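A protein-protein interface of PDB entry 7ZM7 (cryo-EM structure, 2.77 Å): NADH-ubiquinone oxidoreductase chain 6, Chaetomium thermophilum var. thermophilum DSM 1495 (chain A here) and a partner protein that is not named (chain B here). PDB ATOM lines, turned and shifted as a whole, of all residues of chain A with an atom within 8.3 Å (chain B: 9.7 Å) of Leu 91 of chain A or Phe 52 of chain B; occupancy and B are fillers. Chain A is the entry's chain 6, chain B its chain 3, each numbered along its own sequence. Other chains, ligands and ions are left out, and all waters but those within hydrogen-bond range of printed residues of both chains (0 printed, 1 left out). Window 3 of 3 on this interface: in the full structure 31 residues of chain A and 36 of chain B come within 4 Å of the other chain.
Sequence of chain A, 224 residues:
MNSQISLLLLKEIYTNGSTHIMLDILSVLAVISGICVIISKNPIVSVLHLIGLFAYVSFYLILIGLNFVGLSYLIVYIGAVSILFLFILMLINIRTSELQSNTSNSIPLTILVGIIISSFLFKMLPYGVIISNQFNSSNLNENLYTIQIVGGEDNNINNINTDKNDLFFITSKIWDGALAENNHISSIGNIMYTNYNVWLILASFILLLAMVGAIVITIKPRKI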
ATOM      1  N   ILE A  44     -10.219 -12.334  -7.406  1.00  0.00           N
ATOM      2  CA  ILE A  44      -9.082 -11.815  -8.166  1.00  0.00           C
ATOM      3  C   ILE A  44      -8.818 -10.368  -7.790  1.00  0.00           C
ATOM      4  O   ILE A  44      -7.675  -9.960  -7.570  1.00  0.00           O
ATOM      5  CB  ILE A  44      -9.332 -11.952  -9.675  1.00  0.00           C
ATOM      6  CG1 ILE A  44      -9.553 -13.404 -10.072  1.00  0.00           C
ATOM      7  CG2 ILE A  44      -8.165 -11.399 -10.464  1.00  0.00           C
ATOM      8  CD1 ILE A  44      -8.390 -14.253  -9.785  1.00  0.00           C
ATOM      9  N   LEU A  84       1.506 -16.938  -6.353  1.00  0.00           N
ATOM     10  CA  LEU A  84       0.886 -18.230  -6.105  1.00  0.00           C
ATOM     11  C   LEU A  84      -0.616 -18.083  -5.900  1.00  0.00           C
ATOM     12  O   LEU A  84      -1.398 -18.928  -6.345  1.00  0.00           O
ATOM     13  CB  LEU A  84       1.550 -18.893  -4.903  1.00  0.00           C
ATOM     14  CG  LEU A  84       1.389 -20.405  -4.733  1.00  0.00           C
ATOM     15  CD1 LEU A  84       1.529 -21.106  -6.059  1.00  0.00           C
ATOM     16  CD2 LEU A  84       2.377 -20.937  -3.734  1.00  0.00           C
ATOM     17  N   PHE A  85      -1.042 -17.010  -5.231  1.00  0.00           N
ATOM     18  CA  PHE A  85      -2.465 -16.732  -5.095  1.00  0.00           C
ATOM     19  C   PHE A  85      -3.110 -16.458  -6.444  1.00  0.00           C
ATOM     20  O   PHE A  85      -4.243 -16.885  -6.697  1.00  0.00           O
ATOM     21  CB  PHE A  85      -2.681 -15.552  -4.152  1.00  0.00           C
ATOM     22  CG  PHE A  85      -2.807 -15.954  -2.720  1.00  0.00           C
ATOM     23  CD1 PHE A  85      -3.972 -16.537  -2.251  1.00  0.00           C
ATOM     24  CD2 PHE A  85      -1.751 -15.790  -1.847  1.00  0.00           C
ATOM     25  CE1 PHE A  85      -4.075 -16.927  -0.948  1.00  0.00           C
ATOM     26  CE2 PHE A  85      -1.858 -16.175  -0.549  1.00  0.00           C
ATOM     27  CZ  PHE A  85      -3.019 -16.750  -0.098  1.00  0.00           C
ATOM     28  N   LEU A  86      -2.418 -15.733  -7.320  1.00  0.00           N
ATOM     29  CA  LEU A  86      -2.972 -15.473  -8.643  1.00  0.00           C
ATOM     30  C   LEU A  86      -3.081 -16.749  -9.474  1.00  0.00           C
ATOM     31  O   LEU A  86      -4.127 -16.996 -10.076  1.00  0.00           O
ATOM     32  CB  LEU A  86      -2.140 -14.411  -9.350  1.00  0.00           C
ATOM     33  CG  LEU A  86      -2.445 -12.988  -8.881  1.00  0.00           C
ATOM     34  CD1 LEU A  86      -1.366 -12.038  -9.309  1.00  0.00           C
ATOM     35  CD2 LEU A  86      -3.782 -12.530  -9.391  1.00  0.00           C
ATOM     36  N   PHE A  87      -2.033 -17.579  -9.514  1.00  0.00           N
ATOM     37  CA  PHE A  87      -2.160 -18.881 -10.172  1.00  0.00           C
ATOM     38  C   PHE A  87      -3.423 -19.617  -9.755  1.00  0.00           C
ATOM     39  O   PHE A  87      -4.277 -19.923 -10.592  1.00  0.00           O
ATOM     40  CB  PHE A  87      -0.949 -19.781  -9.905  1.00  0.00           C
ATOM     41  CG  PHE A  87       0.305 -19.372 -10.606  1.00  0.00           C
ATOM     42  CD1 PHE A  87       0.274 -18.468 -11.650  1.00  0.00           C
ATOM     43  CD2 PHE A  87       1.506 -19.972 -10.287  1.00  0.00           C
ATOM     44  CE1 PHE A  87       1.427 -18.128 -12.324  1.00  0.00           C
ATOM     45  CE2 PHE A  87       2.662 -19.639 -10.971  1.00  0.00           C
ATOM     46  CZ  PHE A  87       2.622 -18.711 -11.986  1.00  0.00           C
ATOM     47  N   ILE A  88      -3.567 -19.902  -8.466  1.00  0.00           N
ATOM     48  CA  ILE A  88      -4.699 -20.705  -8.032  1.00  0.00           C
ATOM     49  C   ILE A  88      -6.012 -20.008  -8.365  1.00  0.00           C
ATOM     50  O   ILE A  88      -6.970 -20.643  -8.806  1.00  0.00           O
ATOM     51  CB  ILE A  88      -4.581 -21.035  -6.534  1.00  0.00           C
ATOM     52  CG1 ILE A  88      -3.301 -21.813  -6.284  1.00  0.00           C
ATOM     53  CG2 ILE A  88      -5.774 -21.829  -6.063  1.00  0.00           C
ATOM     54  CD1 ILE A  88      -3.244 -23.100  -7.041  1.00  0.00           C
ATOM     55  N   LEU A  89      -6.074 -18.698  -8.183  1.00  0.00           N
ATOM     56  CA  LEU A  89      -7.344 -18.023  -8.373  1.00  0.00           C
ATOM     57  C   LEU A  89      -7.717 -17.871  -9.839  1.00  0.00           C
ATOM     58  O   LEU A  89      -8.887 -17.644 -10.146  1.00  0.00           O
ATOM     59  CB  LEU A  89      -7.307 -16.666  -7.698  1.00  0.00           C
ATOM     60  CG  LEU A  89      -7.571 -16.557  -6.204  1.00  0.00           C
ATOM     61  CD1 LEU A  89      -7.798 -15.111  -5.877  1.00  0.00           C
ATOM     62  CD2 LEU A  89      -8.746 -17.377  -5.795  1.00  0.00           C
ATOM     63  N   MET A  90      -6.762 -17.992 -10.749  1.00  0.00           N
ATOM     64  CA  MET A  90      -7.040 -17.906 -12.173  1.00  0.00           C
ATOM     65  C   MET A  90      -7.169 -19.273 -12.823  1.00  0.00           C
ATOM     66  O   MET A  90      -7.186 -19.356 -14.047  1.00  0.00           O
ATOM     67  CB  MET A  90      -5.959 -17.076 -12.868  1.00  0.00           C
ATOM     68  CG  MET A  90      -5.940 -15.648 -12.361  1.00  0.00           C
ATOM     69  SD  MET A  90      -4.439 -14.682 -12.598  1.00  0.00           S
ATOM     70  CE  MET A  90      -3.799 -15.356 -14.095  1.00  0.00           C
ATOM     71  N   LEU A  91      -7.262 -20.332 -12.042  1.00  0.00           N
ATOM     72  CA  LEU A  91      -7.429 -21.691 -12.531  1.00  0.00           C
ATOM     73  C   LEU A  91      -8.590 -22.410 -11.876  1.00  0.00           C
ATOM     74  O   LEU A  91      -9.279 -23.185 -12.531  1.00  0.00           O
ATOM     75  CB  LEU A  91      -6.160 -22.490 -12.291  1.00  0.00           C
ATOM     76  CG  LEU A  91      -4.933 -22.082 -13.073  1.00  0.00           C
ATOM     77  CD1 LEU A  91      -3.722 -22.711 -12.423  1.00  0.00           C
ATOM     78  CD2 LEU A  91      -5.089 -22.536 -14.502  1.00  0.00           C
ATOM     79  N   ILE A  92      -8.806 -22.188 -10.582  1.00  0.00           N
ATOM     80  CA  ILE A  92     -10.035 -22.633  -9.952  1.00  0.00           C
ATOM     81  C   ILE A  92     -11.216 -21.958 -10.624  1.00  0.00           C
ATOM     82  O   ILE A  92     -11.183 -20.761 -10.936  1.00  0.00           O
ATOM     83  CB  ILE A  92      -9.994 -22.330  -8.447  1.00  0.00           C
ATOM     84  CG1 ILE A  92      -9.065 -23.312  -7.742  1.00  0.00           C
ATOM     85  CG2 ILE A  92     -11.370 -22.344  -7.860  1.00  0.00           C
ATOM     86  CD1 ILE A  92      -9.120 -23.212  -6.242  1.00  0.00           C
ATOM     87  N   ASN A  93     -12.252 -22.733 -10.895  1.00  0.00           N
ATOM     88  CA  ASN A  93     -13.485 -22.152 -11.393  1.00  0.00           C
ATOM     89  C   ASN A  93     -14.172 -21.413 -10.259  1.00  0.00           C
ATOM     90  O   ASN A  93     -14.409 -21.982  -9.193  1.00  0.00           O
ATOM     91  CB  ASN A  93     -14.379 -23.240 -11.977  1.00  0.00           C
ATOM     92  CG  ASN A  93     -13.849 -23.776 -13.282  1.00  0.00           C
ATOM     93  OD1 ASN A  93     -13.396 -24.914 -13.363  1.00  0.00           O
ATOM     94  ND2 ASN A  93     -13.901 -22.952 -14.321  1.00  0.00           N
ATOM     95  N   ILE A  94     -14.463 -20.140 -10.469  1.00  0.00           N
ATOM     96  CA  ILE A  94     -15.095 -19.306  -9.461  1.00  0.00           C
ATOM     97  C   ILE A  94     -16.326 -18.670 -10.076  1.00  0.00           C
ATOM     98  O   ILE A  94     -16.218 -17.856 -11.001  1.00  0.00           O
ATOM     99  CB  ILE A  94     -14.140 -18.232  -8.925  1.00  0.00           C
ATOM    100  CG1 ILE A  94     -12.936 -18.869  -8.239  1.00  0.00           C
ATOM    101  CG2 ILE A  94     -14.872 -17.316  -7.969  1.00  0.00           C
ATOM    102  CD1 ILE A  94     -11.637 -18.178  -8.526  1.00  0.00           C
ATOM    103  N   THR A 218      -0.433 -33.097  -3.032  1.00  0.00           N
ATOM    104  CA  THR A 218      -0.957 -32.637  -4.309  1.00  0.00           C
ATOM    105  C   THR A 218      -0.620 -33.561  -5.467  1.00  0.00           C
ATOM    106  O   THR A 218      -1.493 -33.838  -6.289  1.00  0.00           O
ATOM    107  CB  THR A 218      -0.482 -31.198  -4.618  1.00  0.00           C
ATOM    108  OG1 THR A 218       0.919 -31.072  -4.363  1.00  0.00           O
ATOM    109  CG2 THR A 218      -1.253 -30.187  -3.796  1.00  0.00           C
ATOM    110  N   SER B  48     -16.859 -23.089 -19.677  1.00  0.00           N
ATOM    111  CA  SER B  48     -16.546 -24.511 -19.673  1.00  0.00           C
ATOM    112  C   SER B  48     -15.594 -24.795 -18.523  1.00  0.00           C
ATOM    113  O   SER B  48     -14.941 -23.891 -17.996  1.00  0.00           O
ATOM    114  CB  SER B  48     -15.937 -24.959 -21.006  1.00  0.00           C
ATOM    115  OG  SER B  48     -14.769 -24.215 -21.307  1.00  0.00           O
ATOM    116  N   ARG B  49     -15.519 -26.066 -18.142  1.00  0.00           N
ATOM    117  CA  ARG B  49     -14.639 -26.497 -17.065  1.00  0.00           C
ATOM    118  C   ARG B  49     -13.628 -27.490 -17.604  1.00  0.00           C
ATOM    119  O   ARG B  49     -13.990 -28.444 -18.298  1.00  0.00           O
ATOM    120  CB  ARG B  49     -15.415 -27.142 -15.918  1.00  0.00           C
ATOM    121  CG  ARG B  49     -16.465 -26.242 -15.299  1.00  0.00           C
ATOM    122  CD  ARG B  49     -16.751 -26.680 -13.887  1.00  0.00           C
ATOM    123  NE  ARG B  49     -15.503 -26.735 -13.141  1.00  0.00           N
ATOM    124  CZ  ARG B  49     -15.390 -27.056 -11.859  1.00  0.00           C
ATOM    125  NH1 ARG B  49     -16.464 -27.361 -11.147  1.00  0.00           N
ATOM    126  NH2 ARG B  49     -14.192 -27.066 -11.297  1.00  0.00           N
ATOM    127  N   SER B  50     -12.355 -27.253 -17.294  1.00  0.00           N
ATOM    128  CA  SER B  50     -11.344 -28.258 -17.537  1.00  0.00           C
ATOM    129  C   SER B  50     -10.441 -28.253 -16.325  1.00  0.00           C
ATOM    130  O   SER B  50     -10.181 -27.181 -15.767  1.00  0.00           O
ATOM    131  CB  SER B  50     -10.527 -28.016 -18.809  1.00  0.00           C
ATOM    132  OG  SER B  50     -11.298 -28.268 -19.973  1.00  0.00           O
ATOM    133  N   PRO B  51      -9.973 -29.414 -15.887  1.00  0.00           N
ATOM    134  CA  PRO B  51      -9.037 -29.446 -14.764  1.00  0.00           C
ATOM    135  C   PRO B  51      -7.775 -28.682 -15.107  1.00  0.00           C
ATOM    136  O   PRO B  51      -7.292 -28.725 -16.237  1.00  0.00           O
ATOM    137  CB  PRO B  51      -8.748 -30.939 -14.576  1.00  0.00           C
ATOM    138  CG  PRO B  51      -9.741 -31.651 -15.393  1.00  0.00           C
ATOM    139  CD  PRO B  51     -10.176 -30.739 -16.479  1.00  0.00           C
ATOM    140  N   PHE B  52      -7.235 -27.986 -14.121  1.00  0.00           N
ATOM    141  CA  PHE B  52      -5.940 -27.353 -14.292  1.00  0.00           C
ATOM    142  C   PHE B  52      -4.845 -28.299 -13.834  1.00  0.00           C
ATOM    143  O   PHE B  52      -5.042 -29.125 -12.940  1.00  0.00           O
ATOM    144  CB  PHE B  52      -5.863 -26.023 -13.533  1.00  0.00           C
ATOM    145  CG  PHE B  52      -5.683 -26.159 -12.048  1.00  0.00           C
ATOM    146  CD1 PHE B  52      -6.763 -26.333 -11.226  1.00  0.00           C
ATOM    147  CD2 PHE B  52      -4.435 -26.057 -11.479  1.00  0.00           C
ATOM    148  CE1 PHE B  52      -6.597 -26.439  -9.874  1.00  0.00           C
ATOM    149  CE2 PHE B  52      -4.261 -26.169 -10.120  1.00  0.00           C
ATOM    150  CZ  PHE B  52      -5.340 -26.355  -9.316  1.00  0.00           C
ATOM    151  N   ASN B  53      -3.692 -28.187 -14.478  1.00  0.00           N
ATOM    152  CA  ASN B  53      -2.573 -29.069 -14.186  1.00  0.00           C
ATOM    153  C   ASN B  53      -1.930 -28.692 -12.860  1.00  0.00           C
ATOM    154  O   ASN B  53      -1.818 -27.513 -12.519  1.00  0.00           O
ATOM    155  CB  ASN B  53      -1.563 -29.007 -15.324  1.00  0.00           C
ATOM    156  CG  ASN B  53      -2.233 -29.104 -16.683  1.00  0.00           C
ATOM    157  OD1 ASN B  53      -2.687 -30.173 -17.083  1.00  0.00           O
ATOM    158  ND2 ASN B  53      -2.324 -27.977 -17.391  1.00  0.00           N
ATOM    159  N   ILE B  54      -1.516 -29.703 -12.095  1.00  0.00           N
ATOM    160  CA  ILE B  54      -0.997 -29.417 -10.767  1.00  0.00           C
ATOM    161  C   ILE B  54       0.385 -28.789 -10.825  1.00  0.00           C
ATOM    162  O   ILE B  54       0.813 -28.157  -9.859  1.00  0.00           O
ATOM    163  CB  ILE B  54      -1.016 -30.683  -9.883  1.00  0.00           C
ATOM    164  CG1 ILE B  54      -0.790 -30.298  -8.427  1.00  0.00           C
ATOM    165  CG2 ILE B  54       0.047 -31.648 -10.313  1.00  0.00           C
ATOM    166  CD1 ILE B  54      -1.825 -29.395  -7.901  1.00  0.00           C
ATOM    167  N   SER B  55       1.076 -28.902 -11.953  1.00  0.00           N
ATOM    168  CA  SER B  55       2.445 -28.416 -12.041  1.00  0.00           C
ATOM    169  C   SER B  55       2.519 -26.901 -11.923  1.00  0.00           C
ATOM    170  O   SER B  55       3.549 -26.365 -11.508  1.00  0.00           O
ATOM    171  CB  SER B  55       3.082 -28.899 -13.343  1.00  0.00           C
ATOM    172  OG  SER B  55       2.413 -28.378 -14.467  1.00  0.00           O
ATOM    173  N   PHE B  56       1.442 -26.195 -12.273  1.00  0.00           N
ATOM    174  CA  PHE B  56       1.389 -24.757 -12.033  1.00  0.00           C
ATOM    175  C   PHE B  56       1.523 -24.439 -10.555  1.00  0.00           C
ATOM    176  O   PHE B  56       2.211 -23.490 -10.173  1.00  0.00           O
ATOM    177  CB  PHE B  56       0.089 -24.182 -12.572  1.00  0.00           C
ATOM    178  CG  PHE B  56       0.106 -23.962 -14.038  1.00  0.00           C
ATOM    179  CD1 PHE B  56       1.121 -23.228 -14.617  1.00  0.00           C
ATOM    180  CD2 PHE B  56      -0.884 -24.493 -14.842  1.00  0.00           C
ATOM    181  CE1 PHE B  56       1.151 -23.034 -15.961  1.00  0.00           C
ATOM    182  CE2 PHE B  56      -0.856 -24.300 -16.198  1.00  0.00           C
ATOM    183  CZ  PHE B  56       0.159 -23.563 -16.755  1.00  0.00           C
ATOM    184  N   PHE B  57       0.851 -25.211  -9.708  1.00  0.00           N
ATOM    185  CA  PHE B  57       0.980 -25.008  -8.277  1.00  0.00           C
ATOM    186  C   PHE B  57       2.404 -25.269  -7.821  1.00  0.00           C
ATOM    187  O   PHE B  57       2.946 -24.522  -7.004  1.00  0.00           O
ATOM    188  CB  PHE B  57      -0.019 -25.899  -7.533  1.00  0.00           C
ATOM    189  CG  PHE B  57       0.146 -25.869  -6.062  1.00  0.00           C
ATOM    190  CD1 PHE B  57      -0.106 -24.710  -5.355  1.00  0.00           C
ATOM    191  CD2 PHE B  57       0.593 -26.978  -5.381  1.00  0.00           C
ATOM    192  CE1 PHE B  57       0.074 -24.663  -3.999  1.00  0.00           C
ATOM    193  CE2 PHE B  57       0.768 -26.939  -4.036  1.00  0.00           C
ATOM    194  CZ  PHE B  57       0.508 -25.774  -3.343  1.00  0.00           C
ATOM    195  N   ILE B  58       3.031 -26.311  -8.354  1.00  0.00           N
ATOM    196  CA  ILE B  58       4.363 -26.696  -7.906  1.00  0.00           C
ATOM    197  C   ILE B  58       5.396 -25.647  -8.298  1.00  0.00           C
ATOM    198  O   ILE B  58       6.357 -25.409  -7.567  1.00  0.00           O
ATOM    199  CB  ILE B  58       4.721 -28.087  -8.454  1.00  0.00           C
ATOM    200  CG1 ILE B  58       3.563 -29.071  -8.244  1.00  0.00           C
ATOM    201  CG2 ILE B  58       6.015 -28.593  -7.833  1.00  0.00           C
ATOM    202  CD1 ILE B  58       3.051 -29.147  -6.865  1.00  0.00           C
ATOM    203  N   TYR B  59       5.227 -25.013  -9.454  1.00  0.00           N
ATOM    204  CA  TYR B  59       6.145 -23.956  -9.857  1.00  0.00           C
ATOM    205  C   TYR B  59       6.136 -22.814  -8.854  1.00  0.00           C
ATOM    206  O   TYR B  59       7.192 -22.335  -8.435  1.00  0.00           O
ATOM    207  CB  TYR B  59       5.779 -23.454 -11.254  1.00  0.00           C
ATOM    208  CG  TYR B  59       6.023 -24.474 -12.324  1.00  0.00           C
ATOM    209  CD1 TYR B  59       6.915 -25.496 -12.126  1.00  0.00           C
ATOM    210  CD2 TYR B  59       5.288 -24.471 -13.500  1.00  0.00           C
ATOM    211  CE1 TYR B  59       7.127 -26.441 -13.081  1.00  0.00           C
ATOM    212  CE2 TYR B  59       5.489 -25.427 -14.459  1.00  0.00           C
ATOM    213  CZ  TYR B  59       6.414 -26.405 -14.240  1.00  0.00           C
ATOM    214  OH  TYR B  59       6.635 -27.373 -15.183  1.00  0.00           O
ATOM    215  N   GLY B  60       4.948 -22.376  -8.445  1.00  0.00           N
ATOM    216  CA  GLY B  60       4.861 -21.284  -7.490  1.00  0.00           C
ATOM    217  C   GLY B  60       5.365 -21.661  -6.110  1.00  0.00           C
ATOM    218  O   GLY B  60       5.971 -20.842  -5.417  1.00  0.00           O
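The guanidinium group (NE) of Arg 49 of chain B is in hydrogen-bond range of the side-chain amide oxygen (OD1) of Asn 93 of chain A (2.8 Å).
Leu 84 of chain A touches Phe 57 of chain B (CD1 to O, 3.8 Å).
CA of Gly 60 of chain B touches CD1 of Leu 84 of chain A, at 3.6 Å.
O of Phe 56 of chain B touches CD2 of Phe 87 of chain A, at 3.6 Å.
Ile 88 of chain A touches Phe 57 of chain B (CD1 to CD1, 3.9 Å).
Phe 52 of chain B touches Leu 91 of chain A.
Asn 93 of chain A touches Ser 48 of chain B (ND2 to O, 3.9 Å).
CG1 of Ile 54 of chain B touches CB of Thr 218 of chain A, at 3.9 Å.
Phe 57 of chain B touches Thr 218 of chain A.
Thr 218 of chain A touches Ile 58 of chain B (OG1 to CD1, 3.8 Å).
Of the printed residues of chain B, Leu 91 of chain A touches Phe 52.
Of the printed residues of chain A, Phe 52 of chain B touches Leu 91.
No residue of chain B comes within 4 Å of Ile 92 of chain A.
Printed residues of chain B within 4 Å of Asn 93 of chain A: Ser 48 (3.9 Å) and Arg 49 (2.8 Å).
Of the printed residues of chain B, Leu 84 of chain A touches Phe 57 (3.8 Å) and Gly 60 (3.6 Å).
Of the printed residues of chain A, Ile 58 of chain B touches Thr 218.
Of the printed residues of chain A, Phe 57 of chain B touches Leu 84, Ile 88 and Thr 218.
Of the printed residues of chain A, Phe 56 of chain B touches Phe 87 (3.6 Å).
Ser 55 of chain B touches none of the printed residues of chain A.
Ile 94 of chain A touches none of the printed residues of chain B.
The nearest residue of chain A that does not touch Phe 52 of chain B is Ile 88 of chain A (4.5 Å).
The nearest printed residue of chain A that does not touch Ile 58 of chain B is Leu 84 of chain A (5.9 Å).
Of the 13 printed residues of chain B, 8 touch a printed residue of chain A.
Among the printed residues, 10 pairs touch across the chains.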
